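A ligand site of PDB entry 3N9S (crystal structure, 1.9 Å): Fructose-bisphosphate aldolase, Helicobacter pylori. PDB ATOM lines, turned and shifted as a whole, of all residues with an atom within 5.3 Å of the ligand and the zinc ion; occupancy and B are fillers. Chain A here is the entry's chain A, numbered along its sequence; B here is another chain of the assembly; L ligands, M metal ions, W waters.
The zinc ion is bound by O1 of the ligand. A ring nitrogen (NE2) of His 180 is bound to the zinc ion, 2.1 Å away. ND1 of His 210 is bound to the zinc ion. NE2 of His 83 binds the zinc ion. O6 of the ligand is bound to the zinc ion, 2.6 Å away.
Residues that only touch the zinc ion: Asn 253. Within 4 Å of the zinc ion: His 83, His 180, His 210 and Asn 253.
Merely in contact with the ligand: Asn 23 (3.2 Å) and Thr 254 (3.8 Å). Hydrophobic or aromatic side chains within 4 Å of the ligand: His 83, His 180 and His 210. Of the 24 residues printed, 16 come within 4 Å of the ligand. Along chain A the residues within 4 Å of the ligand span positions 23 to 256.
Water W6 lies within hydrogen-bond range of an oxygen (O4) of the ligand (2.6 Å) and the backbone NH of Gly 51 (3.0 Å). Water W7 bridges O9 of the ligand (2.8 Å) and OD2 of Asp 255 (2.8 Å). Water W2 lies within hydrogen-bond range of O3 of the ligand and OG of Ser 49. Water W5 bridges OD2 of Asp 255 (2.4 Å) and O2 of the ligand (3.0 Å).
The backbone NH of Thr 256 is in hydrogen-bond range of an oxygen (O10) of the ligand, 2.8 Å away. The backbone NH (N) of Ala 212 lies within hydrogen-bond range of an oxygen (O8) of the ligand, at 3.1 Å. The backbone NH of Asp 255 lies within hydrogen-bond range of an oxygen (O10) of the ligand (2.9 Å). An oxygen (O3) of the ligand is in salt-bridge range of the guanidinium group (NH1) of Arg 280 of chain B (2.7 Å). An oxygen (O3) of the ligand sits at hydrogen-bond distance from the side-chain hydroxyl (OG) of Ser 49 (2.6 Å). The side-chain hydroxyl (OG) of Ser 213 lies within hydrogen-bond range of an oxygen (O10) of the ligand, at 2.6 Å. An oxygen (O8) of the ligand is in salt-bridge range of the side-chain amino group of Lys 184 (2.6 Å). The backbone NH (N) of Gly 211 lies close to an oxygen (O7) of the ligand (3.1 Å). The backbone NH (N) of Gly 181 is in hydrogen-bond range of an oxygen (O9) of the ligand. The backbone NH (N) of Ser 213 is in hydrogen-bond range of an oxygen (O8) of the ligand, at 2.8 Å. O1 of the ligand lies close to ND2 of Asn 253, 3.1 Å away. The side-chain hydroxyl of Thr 256 is in hydrogen-bond range of an oxygen (O9) of the ligand (2.7 Å). The side-chain carboxylate of Asp 82 sits close to an oxygen (O1) of the ligand (2.7 Å).
N of Asn 23 is in hydrogen-bond range of O of Thr 254 (3.5 Å). NE of Arg 280 of chain B lies within salt-bridge range of OD1 of Asp 278 of chain B. The side-chain amide oxygen (OD1) of Asn 23 sits at hydrogen-bond distance from the side-chain amide nitrogen (NE2) of Gln 47 (3.0 Å). The side-chain carboxylate (OD2) of Asp 82 is in hydrogen-bond range of the side-chain amide nitrogen (NE2) of Gln 47, 3.5 Å away. The backbone NH (N) of Ala 52 lies within hydrogen-bond range of the side-chain hydroxyl (OG) of Ser 49 (3.0 Å). The side-chain hydroxyl (OG) of Ser 213 lies within hydrogen-bond range of the backbone NH (N) of Thr 256 (3.3 Å). The backbone carbonyl oxygen (O) of Gly 211 sits close to the side-chain amino group (NZ) of Lys 184, 3.2 Å away. The side-chain carboxylate (OD2) of Asp 82 lies within hydrogen-bond range of the side-chain amide nitrogen (ND2) of Asn 23 (3.2 Å).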
ATOM      1  N   ASN A  23       7.588 -15.814 -25.691  1.00  0.00           N
ATOM      2  CA  ASN A  23       8.241 -14.869 -24.789  1.00  0.00           C
ATOM      3  C   ASN A  23       9.560 -15.438 -24.306  1.00  0.00           C
ATOM      4  O   ASN A  23       9.732 -16.667 -24.192  1.00  0.00           O
ATOM      5  CB  ASN A  23       7.335 -14.526 -23.601  1.00  0.00           C
ATOM      6  CG  ASN A  23       6.172 -13.629 -23.984  1.00  0.00           C
ATOM      7  OD1 ASN A  23       5.238 -14.069 -24.643  1.00  0.00           O
ATOM      8  ND2 ASN A  23       6.222 -12.375 -23.568  1.00  0.00           N
ATOM      9  N   GLN A  47       9.159 -12.353 -28.449  1.00  0.00           N
ATOM     10  CA  GLN A  47       8.674 -11.205 -27.680  1.00  0.00           C
ATOM     11  C   GLN A  47       9.236 -11.065 -26.273  1.00  0.00           C
ATOM     12  O   GLN A  47       9.590 -12.048 -25.617  1.00  0.00           O
ATOM     13  CB  GLN A  47       7.157 -11.139 -27.617  1.00  0.00           C
ATOM     14  CG  GLN A  47       6.354 -12.397 -27.849  1.00  0.00           C
ATOM     15  CD  GLN A  47       4.870 -12.096 -27.933  1.00  0.00           C
ATOM     16  OE1 GLN A  47       4.396 -11.480 -28.896  1.00  0.00           O
ATOM     17  NE2 GLN A  47       4.118 -12.506 -26.920  1.00  0.00           N
ATOM     18  N   SER A  49       8.212  -8.848 -22.697  1.00  0.00           N
ATOM     19  CA  SER A  49       7.366  -7.917 -21.963  1.00  0.00           C
ATOM     20  C   SER A  49       8.209  -6.797 -21.353  1.00  0.00           C
ATOM     21  O   SER A  49       9.442  -6.843 -21.332  1.00  0.00           O
ATOM     22  CB  SER A  49       6.677  -8.686 -20.840  1.00  0.00           C
ATOM     23  OG  SER A  49       7.668  -9.133 -19.918  1.00  0.00           O
ATOM     24  N   GLY A  51       8.463  -6.178 -18.192  1.00  0.00           N
ATOM     25  CA  GLY A  51       9.144  -6.803 -17.066  1.00  0.00           C
ATOM     26  C   GLY A  51      10.345  -7.633 -17.484  1.00  0.00           C
ATOM     27  O   GLY A  51      11.313  -7.745 -16.725  1.00  0.00           O
ATOM     28  N   ALA A  52      10.293  -8.238 -18.657  1.00  0.00           N
ATOM     29  CA  ALA A  52      11.424  -9.011 -19.164  1.00  0.00           C
ATOM     30  C   ALA A  52      12.528  -8.059 -19.625  1.00  0.00           C
ATOM     31  O   ALA A  52      13.711  -8.345 -19.471  1.00  0.00           O
ATOM     32  CB  ALA A  52      10.998  -9.899 -20.312  1.00  0.00           C
ATOM     33  N   ASP A  82       5.958  -6.936 -26.028  1.00  0.00           N
ATOM     34  CA  ASP A  82       4.693  -7.487 -25.571  1.00  0.00           C
ATOM     35  C   ASP A  82       4.102  -6.585 -24.498  1.00  0.00           C
ATOM     36  O   ASP A  82       4.798  -6.135 -23.589  1.00  0.00           O
ATOM     37  CB  ASP A  82       4.907  -8.906 -25.028  1.00  0.00           C
ATOM     38  CG  ASP A  82       3.607  -9.663 -24.814  1.00  0.00           C
ATOM     39  OD1 ASP A  82       2.569  -9.294 -25.405  1.00  0.00           O
ATOM     40  OD2 ASP A  82       3.630 -10.647 -24.052  1.00  0.00           O
ATOM     41  N   HIS A  83       2.805  -6.318 -24.616  1.00  0.00           N
ATOM     42  CA  HIS A  83       2.098  -5.480 -23.651  1.00  0.00           C
ATOM     43  C   HIS A  83       2.836  -4.193 -23.261  1.00  0.00           C
ATOM     44  O   HIS A  83       3.059  -3.932 -22.085  1.00  0.00           O
ATOM     45  CB  HIS A  83       1.762  -6.292 -22.400  1.00  0.00           C
ATOM     46  CG  HIS A  83       0.743  -7.358 -22.657  1.00  0.00           C
ATOM     47  ND1 HIS A  83      -0.590  -7.071 -22.864  1.00  0.00           N
ATOM     48  CD2 HIS A  83       0.856  -8.698 -22.785  1.00  0.00           C
ATOM     49  CE1 HIS A  83      -1.245  -8.184 -23.092  1.00  0.00           C
ATOM     50  NE2 HIS A  83      -0.399  -9.187 -23.044  1.00  0.00           N
ATOM     51  N   LEU A 138      -9.000  -9.500 -21.202  1.00  0.00           N
ATOM     52  CA  LEU A 138      -8.447 -10.857 -21.289  1.00  0.00           C
ATOM     53  C   LEU A 138      -8.792 -11.684 -20.065  1.00  0.00           C
ATOM     54  O   LEU A 138      -7.899 -12.108 -19.334  1.00  0.00           O
ATOM     55  CB  LEU A 138      -6.932 -10.797 -21.413  1.00  0.00           C
ATOM     56  CG  LEU A 138      -6.359 -10.760 -22.813  1.00  0.00           C
ATOM     57  CD1 LEU A 138      -4.841 -10.657 -22.714  1.00  0.00           C
ATOM     58  CD2 LEU A 138      -6.783 -11.991 -23.605  1.00  0.00           C
ATOM     59  N   SER A 179      -7.244 -15.887 -21.424  1.00  0.00           N
ATOM     60  CA  SER A 179      -6.607 -15.039 -20.430  1.00  0.00           C
ATOM     61  C   SER A 179      -5.205 -15.569 -20.201  1.00  0.00           C
ATOM     62  O   SER A 179      -4.892 -16.701 -20.597  1.00  0.00           O
ATOM     63  CB  SER A 179      -7.405 -15.063 -19.123  1.00  0.00           C
ATOM     64  OG  SER A 179      -7.452 -16.373 -18.602  1.00  0.00           O
ATOM     65  N   HIS A 180      -4.353 -14.765 -19.582  1.00  0.00           N
ATOM     66  CA  HIS A 180      -2.983 -15.169 -19.315  1.00  0.00           C
ATOM     67  C   HIS A 180      -2.892 -16.218 -18.220  1.00  0.00           C
ATOM     68  O   HIS A 180      -3.691 -16.211 -17.275  1.00  0.00           O
ATOM     69  CB  HIS A 180      -2.151 -13.970 -18.902  1.00  0.00           C
ATOM     70  CG  HIS A 180      -1.952 -12.985 -20.010  1.00  0.00           C
ATOM     71  ND1 HIS A 180      -1.835 -11.635 -19.785  1.00  0.00           N
ATOM     72  CD2 HIS A 180      -1.855 -13.157 -21.340  1.00  0.00           C
ATOM     73  CE1 HIS A 180      -1.662 -11.016 -20.934  1.00  0.00           C
ATOM     74  NE2 HIS A 180      -1.678 -11.917 -21.899  1.00  0.00           N
ATOM     75  N   GLY A 181      -1.932 -17.114 -18.342  1.00  0.00           N
ATOM     76  CA  GLY A 181      -1.563 -17.990 -17.252  1.00  0.00           C
ATOM     77  C   GLY A 181      -2.137 -19.391 -17.344  1.00  0.00           C
ATOM     78  O   GLY A 181      -2.827 -19.748 -18.302  1.00  0.00           O
ATOM     79  N   LYS A 184      -6.962 -20.949 -17.053  1.00  0.00           N
ATOM     80  CA  LYS A 184      -7.811 -20.264 -18.027  1.00  0.00           C
ATOM     81  C   LYS A 184      -9.294 -20.563 -17.876  1.00  0.00           C
ATOM     82  O   LYS A 184     -10.124 -19.701 -18.124  1.00  0.00           O
ATOM     83  CB  LYS A 184      -7.385 -20.610 -19.462  1.00  0.00           C
ATOM     84  CG  LYS A 184      -5.950 -20.177 -19.776  1.00  0.00           C
ATOM     85  CD  LYS A 184      -5.606 -20.318 -21.263  1.00  0.00           C
ATOM     86  CE  LYS A 184      -4.084 -20.338 -21.454  1.00  0.00           C
ATOM     87  NZ  LYS A 184      -3.435 -19.133 -20.825  1.00  0.00           N
ATOM     88  N   LEU A 209      -4.013 -13.753 -30.842  1.00  0.00           N
ATOM     89  CA  LEU A 209      -4.635 -14.407 -29.692  1.00  0.00           C
ATOM     90  C   LEU A 209      -3.672 -14.405 -28.505  1.00  0.00           C
ATOM     91  O   LEU A 209      -2.618 -15.039 -28.577  1.00  0.00           O
ATOM     92  CB  LEU A 209      -4.999 -15.851 -30.044  1.00  0.00           C
ATOM     93  CG  LEU A 209      -5.729 -16.645 -28.962  1.00  0.00           C
ATOM     94  CD1 LEU A 209      -7.147 -16.148 -28.815  1.00  0.00           C
ATOM     95  CD2 LEU A 209      -5.712 -18.134 -29.299  1.00  0.00           C
ATOM     96  N   HIS A 210      -4.032 -13.729 -27.431  1.00  0.00           N
ATOM     97  CA  HIS A 210      -3.247 -13.773 -26.185  1.00  0.00           C
ATOM     98  C   HIS A 210      -3.773 -14.893 -25.330  1.00  0.00           C
ATOM     99  O   HIS A 210      -4.892 -15.354 -25.555  1.00  0.00           O
ATOM    100  CB  HIS A 210      -3.384 -12.448 -25.427  1.00  0.00           C
ATOM    101  CG  HIS A 210      -2.629 -11.331 -26.062  1.00  0.00           C
ATOM    102  ND1 HIS A 210      -1.590 -10.675 -25.424  1.00  0.00           N
ATOM    103  CD2 HIS A 210      -2.737 -10.760 -27.281  1.00  0.00           C
ATOM    104  CE1 HIS A 210      -1.099  -9.744 -26.224  1.00  0.00           C
ATOM    105  NE2 HIS A 210      -1.779  -9.776 -27.357  1.00  0.00           N
ATOM    106  N   GLY A 211      -2.977 -15.347 -24.376  1.00  0.00           N
ATOM    107  CA  GLY A 211      -3.406 -16.370 -23.433  1.00  0.00           C
ATOM    108  C   GLY A 211      -3.625 -17.700 -24.127  1.00  0.00           C
ATOM    109  O   GLY A 211      -4.531 -18.450 -23.769  1.00  0.00           O
ATOM    110  N   ALA A 212      -2.778 -18.014 -25.099  1.00  0.00           N
ATOM    111  CA  ALA A 212      -2.980 -19.182 -25.966  1.00  0.00           C
ATOM    112  C   ALA A 212      -2.184 -20.437 -25.583  1.00  0.00           C
ATOM    113  O   ALA A 212      -2.077 -21.367 -26.384  1.00  0.00           O
ATOM    114  CB  ALA A 212      -2.682 -18.793 -27.415  1.00  0.00           C
ATOM    115  N   SER A 213      -1.601 -20.464 -24.388  1.00  0.00           N
ATOM    116  CA  SER A 213      -0.954 -21.694 -23.926  1.00  0.00           C
ATOM    117  C   SER A 213      -1.990 -22.790 -23.779  1.00  0.00           C
ATOM    118  O   SER A 213      -3.157 -22.518 -23.487  1.00  0.00           O
ATOM    119  CB  SER A 213      -0.231 -21.470 -22.606  1.00  0.00           C
ATOM    120  OG  SER A 213       1.035 -20.884 -22.860  1.00  0.00           O
ATOM    121  N   ASN A 253       0.235 -15.899 -29.032  1.00  0.00           N
ATOM    122  CA  ASN A 253       1.120 -15.638 -27.892  1.00  0.00           C
ATOM    123  C   ASN A 253       1.205 -16.814 -26.951  1.00  0.00           C
ATOM    124  O   ASN A 253       0.190 -17.217 -26.360  1.00  0.00           O
ATOM    125  CB  ASN A 253       0.631 -14.427 -27.090  1.00  0.00           C
ATOM    126  CG  ASN A 253       0.803 -13.128 -27.814  1.00  0.00           C
ATOM    127  OD1 ASN A 253       0.943 -13.088 -29.024  1.00  0.00           O
ATOM    128  ND2 ASN A 253       0.773 -12.035 -27.056  1.00  0.00           N
ATOM    129  N   THR A 254       2.422 -17.322 -26.772  1.00  0.00           N
ATOM    130  CA  THR A 254       2.634 -18.532 -25.995  1.00  0.00           C
ATOM    131  C   THR A 254       3.824 -18.291 -25.081  1.00  0.00           C
ATOM    132  O   THR A 254       4.928 -18.043 -25.548  1.00  0.00           O
ATOM    133  CB  THR A 254       2.974 -19.704 -26.906  1.00  0.00           C
ATOM    134  OG1 THR A 254       2.014 -19.759 -27.964  1.00  0.00           O
ATOM    135  CG2 THR A 254       2.964 -21.004 -26.121  1.00  0.00           C
ATOM    136  N   ASP A 255       3.591 -18.409 -23.776  1.00  0.00           N
ATOM    137  CA  ASP A 255       4.586 -18.071 -22.759  1.00  0.00           C
ATOM    138  C   ASP A 255       4.514 -19.109 -21.655  1.00  0.00           C
ATOM    139  O   ASP A 255       5.495 -19.762 -21.325  1.00  0.00           O
ATOM    140  CB  ASP A 255       4.291 -16.673 -22.214  1.00  0.00           C
ATOM    141  CG  ASP A 255       5.101 -16.329 -20.980  1.00  0.00           C
ATOM    142  OD1 ASP A 255       6.322 -16.606 -20.942  1.00  0.00           O
ATOM    143  OD2 ASP A 255       4.518 -15.767 -20.031  1.00  0.00           O
ATOM    144  N   THR A 256       3.328 -19.265 -21.081  1.00  0.00           N
ATOM    145  CA  THR A 256       3.151 -20.172 -19.942  1.00  0.00           C
ATOM    146  C   THR A 256       3.639 -21.608 -20.219  1.00  0.00           C
ATOM    147  O   THR A 256       4.382 -22.168 -19.422  1.00  0.00           O
ATOM    148  CB  THR A 256       1.701 -20.160 -19.476  1.00  0.00           C
ATOM    149  OG1 THR A 256       1.418 -18.881 -18.886  1.00  0.00           O
ATOM    150  CG2 THR A 256       1.448 -21.241 -18.456  1.00  0.00           C
ATOM    151  N   ASP A 257       3.242 -22.192 -21.345  1.00  0.00           N
ATOM    152  CA  ASP A 257       3.690 -23.550 -21.720  1.00  0.00           C
ATOM    153  C   ASP A 257       5.204 -23.690 -21.723  1.00  0.00           C
ATOM    154  O   ASP A 257       5.747 -24.724 -21.306  1.00  0.00           O
ATOM    155  CB  ASP A 257       3.205 -23.940 -23.104  1.00  0.00           C
ATOM    156  CG  ASP A 257       1.746 -24.273 -23.140  1.00  0.00           C
ATOM    157  OD1 ASP A 257       1.159 -24.459 -22.055  1.00  0.00           O
ATOM    158  OD2 ASP A 257       1.199 -24.363 -24.261  1.00  0.00           O
ATOM    159  N   ASP B 278       7.904 -19.017 -12.889  1.00  0.00           N
ATOM    160  CA  ASP B 278       8.460 -17.817 -13.484  1.00  0.00           C
ATOM    161  C   ASP B 278       9.977 -17.894 -13.331  1.00  0.00           C
ATOM    162  O   ASP B 278      10.493 -17.871 -12.201  1.00  0.00           O
ATOM    163  CB  ASP B 278       7.920 -16.570 -12.759  1.00  0.00           C
ATOM    164  CG  ASP B 278       8.439 -15.272 -13.346  1.00  0.00           C
ATOM    165  OD1 ASP B 278       9.421 -15.285 -14.129  1.00  0.00           O
ATOM    166  OD2 ASP B 278       7.873 -14.203 -13.026  1.00  0.00           O
ATOM    167  N   ARG B 280      12.248 -15.830 -13.652  1.00  0.00           N
ATOM    168  CA  ARG B 280      12.868 -14.695 -12.963  1.00  0.00           C
ATOM    169  C   ARG B 280      12.829 -14.860 -11.448  1.00  0.00           C
ATOM    170  O   ARG B 280      13.740 -14.423 -10.739  1.00  0.00           O
ATOM    171  CB  ARG B 280      12.196 -13.393 -13.386  1.00  0.00           C
ATOM    172  CG  ARG B 280      12.467 -13.036 -14.831  1.00  0.00           C
ATOM    173  CD  ARG B 280      11.427 -12.046 -15.345  1.00  0.00           C
ATOM    174  NE  ARG B 280      10.096 -12.644 -15.348  1.00  0.00           N
ATOM    175  CZ  ARG B 280       9.008 -12.047 -15.815  1.00  0.00           C
ATOM    176  NH1 ARG B 280       9.095 -10.827 -16.322  1.00  0.00           N
ATOM    177  NH2 ARG B 280       7.833 -12.671 -15.774  1.00  0.00           N
HETATM  178  O1  LIG L   1       1.126 -11.643 -23.989  1.00  0.00           O
HETATM  179  N1  LIG L   1       1.426 -12.972 -23.707  1.00  0.00           N
HETATM  180  C1  LIG L   1       2.653 -13.236 -22.991  1.00  0.00           C
HETATM  181  C2  LIG L   1       2.525 -12.933 -21.501  1.00  0.00           C
HETATM  182  C3  LIG L   1       3.403 -11.816 -20.976  1.00  0.00           C
HETATM  183  C4  LIG L   1       3.557 -11.754 -19.474  1.00  0.00           C
HETATM  184  O2  LIG L   1       4.863 -11.873 -19.006  1.00  0.00           O
HETATM  185  P1  LIG L   1       5.356 -10.894 -17.791  1.00  0.00           P
HETATM  186  O3  LIG L   1       6.962 -10.654 -17.953  1.00  0.00           O
HETATM  187  O4  LIG L   1       4.557  -9.471 -17.897  1.00  0.00           O
HETATM  188  O5  LIG L   1       5.039 -11.523 -16.515  1.00  0.00           O
HETATM  189  C5  LIG L   1       0.374 -13.962 -23.654  1.00  0.00           C
HETATM  190  O6  LIG L   1      -0.687 -13.728 -24.140  1.00  0.00           O
HETATM  191  C6  LIG L   1       0.747 -15.378 -23.194  1.00  0.00           C
HETATM  192  O7  LIG L   1      -0.331 -16.230 -22.961  1.00  0.00           O
HETATM  193  P2  LIG L   1      -0.163 -17.590 -22.035  1.00  0.00           P
HETATM  194  O8  LIG L   1      -1.467 -18.524 -22.367  1.00  0.00           O
HETATM  195  O9  LIG L   1      -0.083 -17.212 -20.451  1.00  0.00           O
HETATM  196  O10 LIG L   1       1.031 -18.321 -22.454  1.00  0.00           O
HETATM  197 ZN    ZN M   1      -0.709 -11.228 -23.611  1.00  0.00          ZN
HETATM  198  O   HOH W   1       2.219  -9.240 -16.826  1.00  0.00           O
HETATM  199  O   HOH W   2       8.179 -12.512 -19.754  1.00  0.00           O
HETATM  200  O   HOH W   3       3.565 -13.616 -15.586  1.00  0.00           O
HETATM  201  O   HOH W   4       5.081 -10.735 -14.005  1.00  0.00           O
HETATM  202  O   HOH W   5       5.788 -14.649 -18.282  1.00  0.00           O
HETATM  203  O   HOH W   6       5.703  -7.176 -17.727  1.00  0.00           O
HETATM  204  O   HOH W   7       1.822 -15.426 -19.576  1.00  0.00           O
HETATM  205  O   HOH W   8       3.331  -8.356 -20.142  1.00  0.00           O
